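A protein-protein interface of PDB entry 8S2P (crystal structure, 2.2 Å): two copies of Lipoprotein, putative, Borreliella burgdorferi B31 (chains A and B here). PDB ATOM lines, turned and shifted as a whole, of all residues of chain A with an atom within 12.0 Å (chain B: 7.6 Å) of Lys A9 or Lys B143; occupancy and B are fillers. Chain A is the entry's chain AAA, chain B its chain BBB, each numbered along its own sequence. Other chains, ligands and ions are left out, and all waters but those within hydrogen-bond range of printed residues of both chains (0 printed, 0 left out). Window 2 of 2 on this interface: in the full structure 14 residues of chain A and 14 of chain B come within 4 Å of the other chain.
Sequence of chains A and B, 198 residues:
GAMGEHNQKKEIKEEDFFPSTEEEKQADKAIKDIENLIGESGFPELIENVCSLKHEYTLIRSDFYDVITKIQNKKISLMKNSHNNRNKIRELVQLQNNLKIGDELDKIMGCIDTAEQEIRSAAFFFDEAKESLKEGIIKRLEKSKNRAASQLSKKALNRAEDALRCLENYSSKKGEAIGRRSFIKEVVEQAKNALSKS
The side-chain amino group of Lys B145 lies within salt-bridge range of the side-chain carboxylate of Glu B142, at 3.8 Å.
OE1 of Glu A11 lies within salt-bridge range of NZ of Lys A143 (3.8 Å).
Lys A9 touches Lys B143 (O to CG, 3.0 Å).
Ile A12 touches Leu B141 (CG2 to O, 3.4 Å).
Glu A14 touches Glu B142 (CD to OE2, 3.5 Å).
Ile B138 touches Phe A17.
Phe A17 touches Leu B141 (CZ to CB, 3.6 Å).
O of Leu A141 touches CG2 of Ile B12 (3.2 Å).
Lys A143 touches Ile B12.
Lys A9 touches just one residue of chain B: Lys B143 (3.0 Å).
Lys B143 touches one residue of chain A.
Of chain A, only Ile A12 and Phe A17 come within 4 Å of Leu B141.
Of chain A, only Glu A14 comes within 4 Å of Glu B142.
Ser B144 touches none of the printed residues of chain A.
Lys B145 touches none of the printed residues of chain A.
Of the printed residues of chain A, Ile B12 touches Leu A141 and Lys A143.
Of the printed residues of chain B, Phe A17 touches Ile B138 and Leu B141.
Printed residues of chain B within 4 Å of Lys A143: Ile B12 (3.2 Å).
Of the printed residues of chain B, Ile A12 touches Leu B141.
Of the printed residues of chain B, Leu A141 touches Ile B12.
The nearest residue of chain B that does not touch Lys A9 is Leu B141 (4.5 Å).
The nearest residue of chain A that does not touch Lys B143 is Ile A12 (4.2 Å).
The nearest printed residue of chain B that does not touch Phe A17 is Glu B142 (4.6 Å).
Hydrophobic or aromatic side chains of chain A within 4 Å of the printed part of chain B: Ile A12 and Phe A17.
Hydrophobic or aromatic side chains of chain B within 4 Å of the printed part of chain A: Ile B12, Ile B138 and Leu B141.
Among the printed residues, 7 pairs touch across the chains.
Ile A12 touches Leu B141, and with the chains exchanged Leu A141 touches Ile B12.
Lys A143 touches Ile B12, but with the chains exchanged Ile A12 does not touch Lys B143 (4.2 Å).
5 positions are printed for both chains.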
ATOM      1  N   LYS A   9     -11.060  33.095  -5.629  1.00  0.00           N
ATOM      2  CA  LYS A   9     -10.704  34.535  -5.423  1.00  0.00           C
ATOM      3  C   LYS A   9      -9.387  34.608  -4.624  1.00  0.00           C
ATOM      4  O   LYS A   9      -8.515  33.736  -4.846  1.00  0.00           O
ATOM      5  CB  LYS A   9     -11.883  35.250  -4.749  1.00  0.00           C
ATOM      6  CG  LYS A   9     -12.150  36.681  -5.212  1.00  0.00           C
ATOM      7  CD  LYS A   9     -12.525  37.643  -4.093  1.00  0.00           C
ATOM      8  CE  LYS A   9     -13.582  37.103  -3.151  1.00  0.00           C
ATOM      9  NZ  LYS A   9     -13.163  37.239  -1.737  1.00  0.00           N
ATOM     10  N   LYS A  10      -9.225  35.615  -3.751  1.00  0.00           N
ATOM     11  CA  LYS A  10      -8.117  35.705  -2.753  1.00  0.00           C
ATOM     12  C   LYS A  10      -8.516  34.969  -1.457  1.00  0.00           C
ATOM     13  O   LYS A  10      -7.690  34.953  -0.506  1.00  0.00           O
ATOM     14  CB  LYS A  10      -7.753  37.170  -2.478  1.00  0.00           C
ATOM     15  CG  LYS A  10      -6.904  37.856  -3.544  1.00  0.00           C
ATOM     16  CD  LYS A  10      -6.154  39.072  -3.025  1.00  0.00           C
ATOM     17  CE  LYS A  10      -7.041  40.278  -2.792  1.00  0.00           C
ATOM     18  NZ  LYS A  10      -7.005  41.207  -3.946  1.00  0.00           N
ATOM     19  N   GLU A  11      -9.730  34.392  -1.412  1.00  0.00           N
ATOM     20  CA  GLU A  11     -10.203  33.451  -0.353  1.00  0.00           C
ATOM     21  C   GLU A  11      -9.507  32.089  -0.542  1.00  0.00           C
ATOM     22  O   GLU A  11      -8.924  31.581   0.449  1.00  0.00           O
ATOM     23  CB  GLU A  11     -11.734  33.322  -0.397  1.00  0.00           C
ATOM     24  CG  GLU A  11     -12.348  32.666   0.836  1.00  0.00           C
ATOM     25  CD  GLU A  11     -13.873  32.582   0.866  1.00  0.00           C
ATOM     26  OE1 GLU A  11     -14.468  32.067  -0.111  1.00  0.00           O
ATOM     27  OE2 GLU A  11     -14.473  33.013   1.880  1.00  0.00           O
ATOM     28  N   ILE A  12      -9.549  31.542  -1.770  1.00  0.00           N
ATOM     29  CA  ILE A  12      -9.023  30.190  -2.157  1.00  0.00           C
ATOM     30  C   ILE A  12      -7.486  30.194  -2.261  1.00  0.00           C
ATOM     31  O   ILE A  12      -6.949  30.534  -3.324  1.00  0.00           O
ATOM     32  CB  ILE A  12      -9.674  29.685  -3.462  1.00  0.00           C
ATOM     33  CG1 ILE A  12      -9.277  28.238  -3.755  1.00  0.00           C
ATOM     34  CG2 ILE A  12      -9.363  30.597  -4.639  1.00  0.00           C
ATOM     35  CD1 ILE A  12      -9.735  27.267  -2.707  1.00  0.00           C
ATOM     36  N   LYS A  13      -6.815  29.742  -1.202  1.00  0.00           N
ATOM     37  CA  LYS A  13      -5.338  29.773  -1.052  1.00  0.00           C
ATOM     38  C   LYS A  13      -4.762  28.366  -1.271  1.00  0.00           C
ATOM     39  O   LYS A  13      -5.540  27.390  -1.273  1.00  0.00           O
ATOM     40  CB  LYS A  13      -4.980  30.338   0.326  1.00  0.00           C
ATOM     41  CG  LYS A  13      -4.920  31.858   0.389  1.00  0.00           C
ATOM     42  CD  LYS A  13      -3.596  32.424  -0.100  1.00  0.00           C
ATOM     43  CE  LYS A  13      -3.718  33.813  -0.692  1.00  0.00           C
ATOM     44  NZ  LYS A  13      -2.398  34.481  -0.771  1.00  0.00           N
ATOM     45  N   GLU A  14      -3.440  28.287  -1.439  1.00  0.00           N
ATOM     46  CA  GLU A  14      -2.710  27.062  -1.846  1.00  0.00           C
ATOM     47  C   GLU A  14      -2.937  25.957  -0.814  1.00  0.00           C
ATOM     48  O   GLU A  14      -3.221  24.845  -1.254  1.00  0.00           O
ATOM     49  CB  GLU A  14      -1.218  27.344  -2.042  1.00  0.00           C
ATOM     50  CG  GLU A  14      -0.406  26.098  -2.353  1.00  0.00           C
ATOM     51  CD  GLU A  14       0.895  26.335  -3.090  1.00  0.00           C
ATOM     52  OE1 GLU A  14       1.411  27.471  -3.039  1.00  0.00           O
ATOM     53  OE2 GLU A  14       1.385  25.378  -3.723  1.00  0.00           O
ATOM     54  N   GLU A  15      -2.780  26.265   0.483  1.00  0.00           N
ATOM     55  CA  GLU A  15      -2.863  25.308   1.629  1.00  0.00           C
ATOM     56  C   GLU A  15      -4.295  24.777   1.728  1.00  0.00           C
ATOM     57  O   GLU A  15      -4.522  23.697   2.326  1.00  0.00           O
ATOM     58  CB  GLU A  15      -2.400  25.977   2.929  1.00  0.00           C
ATOM     59  CG  GLU A  15      -0.927  25.721   3.239  1.00  0.00           C
ATOM     60  CD  GLU A  15      -0.232  26.671   4.211  1.00  0.00           C
ATOM     61  OE1 GLU A  15      -0.813  27.743   4.523  1.00  0.00           O
ATOM     62  OE2 GLU A  15       0.906  26.343   4.646  1.00  0.00           O
ATOM     63  N   ASP A  16      -5.222  25.514   1.122  1.00  0.00           N
ATOM     64  CA  ASP A  16      -6.651  25.162   1.051  1.00  0.00           C
ATOM     65  C   ASP A  16      -6.822  23.898   0.191  1.00  0.00           C
ATOM     66  O   ASP A  16      -7.824  23.199   0.379  1.00  0.00           O
ATOM     67  CB  ASP A  16      -7.421  26.380   0.535  1.00  0.00           C
ATOM     68  CG  ASP A  16      -8.621  26.730   1.377  1.00  0.00           C
ATOM     69  OD1 ASP A  16      -9.677  26.101   1.171  1.00  0.00           O
ATOM     70  OD2 ASP A  16      -8.479  27.620   2.221  1.00  0.00           O
ATOM     71  N   PHE A  17      -5.906  23.610  -0.740  1.00  0.00           N
ATOM     72  CA  PHE A  17      -5.980  22.397  -1.600  1.00  0.00           C
ATOM     73  C   PHE A  17      -5.357  21.208  -0.880  1.00  0.00           C
ATOM     74  O   PHE A  17      -5.497  20.113  -1.396  1.00  0.00           O
ATOM     75  CB  PHE A  17      -5.313  22.605  -2.966  1.00  0.00           C
ATOM     76  CG  PHE A  17      -6.056  23.590  -3.823  1.00  0.00           C
ATOM     77  CD1 PHE A  17      -5.848  24.953  -3.671  1.00  0.00           C
ATOM     78  CD2 PHE A  17      -7.037  23.160  -4.699  1.00  0.00           C
ATOM     79  CE1 PHE A  17      -6.566  25.865  -4.426  1.00  0.00           C
ATOM     80  CE2 PHE A  17      -7.752  24.072  -5.453  1.00  0.00           C
ATOM     81  CZ  PHE A  17      -7.525  25.422  -5.307  1.00  0.00           C
ATOM     82  N   LEU A 141     -13.986  21.917  -1.190  1.00  0.00           N
ATOM     83  CA  LEU A 141     -13.835  23.257  -1.814  1.00  0.00           C
ATOM     84  C   LEU A 141     -15.177  23.634  -2.442  1.00  0.00           C
ATOM     85  O   LEU A 141     -15.537  24.810  -2.346  1.00  0.00           O
ATOM     86  CB  LEU A 141     -12.667  23.185  -2.795  1.00  0.00           C
ATOM     87  CG  LEU A 141     -11.308  22.956  -2.138  1.00  0.00           C
ATOM     88  CD1 LEU A 141     -10.216  22.793  -3.178  1.00  0.00           C
ATOM     89  CD2 LEU A 141     -10.973  24.089  -1.184  1.00  0.00           C
ATOM     90  N   GLU A 142     -15.868  22.686  -3.085  1.00  0.00           N
ATOM     91  CA  GLU A 142     -17.274  22.940  -3.487  1.00  0.00           C
ATOM     92  C   GLU A 142     -17.854  23.157  -2.103  1.00  0.00           C
ATOM     93  O   GLU A 142     -17.626  22.314  -1.246  1.00  0.00           O
ATOM     94  CB  GLU A 142     -17.866  21.726  -4.192  1.00  0.00           C
ATOM     95  CG  GLU A 142     -17.375  21.508  -5.602  1.00  0.00           C
ATOM     96  CD  GLU A 142     -18.191  20.440  -6.304  1.00  0.00           C
ATOM     97  OE1 GLU A 142     -17.654  19.348  -6.530  1.00  0.00           O
ATOM     98  OE2 GLU A 142     -19.369  20.700  -6.591  1.00  0.00           O
ATOM     99  N   LYS A 143     -18.606  24.208  -1.859  1.00  0.00           N
ATOM    100  CA  LYS A 143     -18.872  24.527  -0.426  1.00  0.00           C
ATOM    101  C   LYS A 143     -20.036  23.823   0.299  1.00  0.00           C
ATOM    102  O   LYS A 143     -20.071  23.941   1.538  1.00  0.00           O
ATOM    103  CB  LYS A 143     -18.959  26.052  -0.308  1.00  0.00           C
ATOM    104  CG  LYS A 143     -17.615  26.765  -0.295  1.00  0.00           C
ATOM    105  CD  LYS A 143     -17.330  27.545  -1.558  1.00  0.00           C
ATOM    106  CE  LYS A 143     -16.022  28.307  -1.493  1.00  0.00           C
ATOM    107  NZ  LYS A 143     -16.004  29.464  -2.419  1.00  0.00           N
ATOM    108  N   ILE B  12     -16.877  29.297  -6.448  1.00  0.00           N
ATOM    109  CA  ILE B  12     -16.144  28.059  -6.884  1.00  0.00           C
ATOM    110  C   ILE B  12     -17.157  26.925  -7.110  1.00  0.00           C
ATOM    111  O   ILE B  12     -18.108  26.797  -6.306  1.00  0.00           O
ATOM    112  CB  ILE B  12     -15.047  27.668  -5.873  1.00  0.00           C
ATOM    113  CG1 ILE B  12     -14.038  26.686  -6.477  1.00  0.00           C
ATOM    114  CG2 ILE B  12     -15.659  27.136  -4.587  1.00  0.00           C
ATOM    115  CD1 ILE B  12     -12.748  26.577  -5.696  1.00  0.00           C
ATOM    116  N   ASP B  16     -14.619  24.165 -12.431  1.00  0.00           N
ATOM    117  CA  ASP B  16     -13.466  25.086 -12.425  1.00  0.00           C
ATOM    118  C   ASP B  16     -12.250  24.246 -12.022  1.00  0.00           C
ATOM    119  O   ASP B  16     -11.134  24.755 -12.117  1.00  0.00           O
ATOM    120  CB  ASP B  16     -13.675  26.247 -11.463  1.00  0.00           C
ATOM    121  CG  ASP B  16     -15.053  26.871 -11.518  1.00  0.00           C
ATOM    122  OD1 ASP B  16     -15.668  26.823 -12.593  1.00  0.00           O
ATOM    123  OD2 ASP B  16     -15.486  27.408 -10.484  1.00  0.00           O
ATOM    124  N   ILE B 138      -4.149  23.943  -9.791  1.00  0.00           N
ATOM    125  CA  ILE B 138      -4.177  24.577  -8.443  1.00  0.00           C
ATOM    126  C   ILE B 138      -3.720  26.034  -8.620  1.00  0.00           C
ATOM    127  O   ILE B 138      -4.429  26.958  -8.149  1.00  0.00           O
ATOM    128  CB  ILE B 138      -3.341  23.764  -7.437  1.00  0.00           C
ATOM    129  CG1 ILE B 138      -4.099  22.515  -6.984  1.00  0.00           C
ATOM    130  CG2 ILE B 138      -2.892  24.617  -6.251  1.00  0.00           C
ATOM    131  CD1 ILE B 138      -3.324  21.637  -6.003  1.00  0.00           C
ATOM    132  N   LYS B 139      -2.634  26.221  -9.368  1.00  0.00           N
ATOM    133  CA  LYS B 139      -1.976  27.532  -9.585  1.00  0.00           C
ATOM    134  C   LYS B 139      -2.948  28.488 -10.299  1.00  0.00           C
ATOM    135  O   LYS B 139      -3.049  29.625  -9.853  1.00  0.00           O
ATOM    136  CB  LYS B 139      -0.643  27.316 -10.306  1.00  0.00           C
ATOM    137  CG  LYS B 139       0.397  28.392 -10.063  1.00  0.00           C
ATOM    138  CD  LYS B 139       0.988  28.364  -8.659  1.00  0.00           C
ATOM    139  CE  LYS B 139       2.131  29.340  -8.493  1.00  0.00           C
ATOM    140  NZ  LYS B 139       2.040  30.087  -7.219  1.00  0.00           N
ATOM    141  N   ARG B 140      -3.744  27.996 -11.243  1.00  0.00           N
ATOM    142  CA  ARG B 140      -4.810  28.832 -11.851  1.00  0.00           C
ATOM    143  C   ARG B 140      -5.849  29.193 -10.779  1.00  0.00           C
ATOM    144  O   ARG B 140      -6.120  30.389 -10.620  1.00  0.00           O
ATOM    145  CB  ARG B 140      -5.518  28.091 -12.987  1.00  0.00           C
ATOM    146  CG  ARG B 140      -6.919  28.601 -13.286  1.00  0.00           C
ATOM    147  CD  ARG B 140      -7.474  28.089 -14.599  1.00  0.00           C
ATOM    148  NE  ARG B 140      -7.705  26.653 -14.605  1.00  0.00           N
ATOM    149  CZ  ARG B 140      -8.776  26.052 -14.104  1.00  0.00           C
ATOM    150  NH1 ARG B 140      -9.738  26.761 -13.542  1.00  0.00           N
ATOM    151  NH2 ARG B 140      -8.881  24.740 -14.168  1.00  0.00           N
ATOM    152  N   LEU B 141      -6.411  28.199 -10.087  1.00  0.00           N
ATOM    153  CA  LEU B 141      -7.446  28.443  -9.047  1.00  0.00           C
ATOM    154  C   LEU B 141      -6.878  29.426  -8.015  1.00  0.00           C
ATOM    155  O   LEU B 141      -7.664  30.230  -7.519  1.00  0.00           O
ATOM    156  CB  LEU B 141      -7.900  27.100  -8.471  1.00  0.00           C
ATOM    157  CG  LEU B 141      -8.661  26.202  -9.444  1.00  0.00           C
ATOM    158  CD1 LEU B 141      -9.051  24.890  -8.790  1.00  0.00           C
ATOM    159  CD2 LEU B 141      -9.891  26.911  -9.984  1.00  0.00           C
ATOM    160  N   GLU B 142      -5.592  29.327  -7.656  1.00  0.00           N
ATOM    161  CA  GLU B 142      -4.975  30.411  -6.853  1.00  0.00           C
ATOM    162  C   GLU B 142      -5.037  31.513  -7.897  1.00  0.00           C
ATOM    163  O   GLU B 142      -4.475  31.329  -8.969  1.00  0.00           O
ATOM    164  CB  GLU B 142      -3.548  30.120  -6.404  1.00  0.00           C
ATOM    165  CG  GLU B 142      -3.284  28.724  -5.877  1.00  0.00           C
ATOM    166  CD  GLU B 142      -1.838  28.537  -5.442  1.00  0.00           C
ATOM    167  OE1 GLU B 142      -1.259  29.492  -4.899  1.00  0.00           O
ATOM    168  OE2 GLU B 142      -1.291  27.445  -5.657  1.00  0.00           O
ATOM    169  N   LYS B 143      -5.669  32.628  -7.624  1.00  0.00           N
ATOM    170  CA  LYS B 143      -5.992  33.553  -8.742  1.00  0.00           C
ATOM    171  C   LYS B 143      -4.849  34.340  -9.426  1.00  0.00           C
ATOM    172  O   LYS B 143      -5.020  34.643 -10.616  1.00  0.00           O
ATOM    173  CB  LYS B 143      -7.109  34.455  -8.220  1.00  0.00           C
ATOM    174  CG  LYS B 143      -8.404  33.729  -7.891  1.00  0.00           C
ATOM    175  CD  LYS B 143      -8.792  32.698  -8.924  1.00  0.00           C
ATOM    176  CE  LYS B 143     -10.051  31.940  -8.565  1.00  0.00           C
ATOM    177  NZ  LYS B 143     -10.812  31.533  -9.771  1.00  0.00           N
ATOM    178  N   SER B 144      -3.732  34.647  -8.768  1.00  0.00           N
ATOM    179  CA  SER B 144      -2.756  35.583  -9.406  1.00  0.00           C
ATOM    180  C   SER B 144      -1.469  34.936  -9.948  1.00  0.00           C
ATOM    181  O   SER B 144      -0.419  35.584  -9.836  1.00  0.00           O
ATOM    182  CB  SER B 144      -2.450  36.730  -8.458  1.00  0.00           C
ATOM    183  OG  SER B 144      -3.633  37.421  -8.093  1.00  0.00           O
ATOM    184  N   LYS B 145      -1.555  33.755 -10.564  1.00  0.00           N
ATOM    185  CA  LYS B 145      -0.335  33.039 -11.035  1.00  0.00           C
ATOM    186  C   LYS B 145      -0.627  32.219 -12.301  1.00  0.00           C
ATOM    187  O   LYS B 145      -0.334  31.019 -12.289  1.00  0.00           O
ATOM    188  CB  LYS B 145       0.194  32.142  -9.914  1.00  0.00           C
ATOM    189  CG  LYS B 145       0.135  32.723  -8.511  1.00  0.00           C
ATOM    190  CD  LYS B 145      -0.738  31.917  -7.581  1.00  0.00           C
ATOM    191  CE  LYS B 145      -0.568  32.309  -6.130  1.00  0.00           C
ATOM    192  NZ  LYS B 145       0.859  32.484  -5.772  1.00  0.00           N
ATOM    193  N   ASN B 146      -1.153  32.845 -13.356  1.00  0.00           N
ATOM    194  CA  ASN B 146      -1.547  32.099 -14.583  1.00  0.00           C
ATOM    195  C   ASN B 146      -0.331  31.838 -15.470  1.00  0.00           C
ATOM    196  O   ASN B 146      -0.428  30.979 -16.342  1.00  0.00           O
ATOM    197  CB  ASN B 146      -2.655  32.805 -15.361  1.00  0.00           C
ATOM    198  CG  ASN B 146      -3.114  32.039 -16.583  1.00  0.00           C
ATOM    199  OD1 ASN B 146      -3.392  30.843 -16.511  1.00  0.00           O
ATOM    200  ND2 ASN B 146      -3.198  32.721 -17.713  1.00  0.00           N
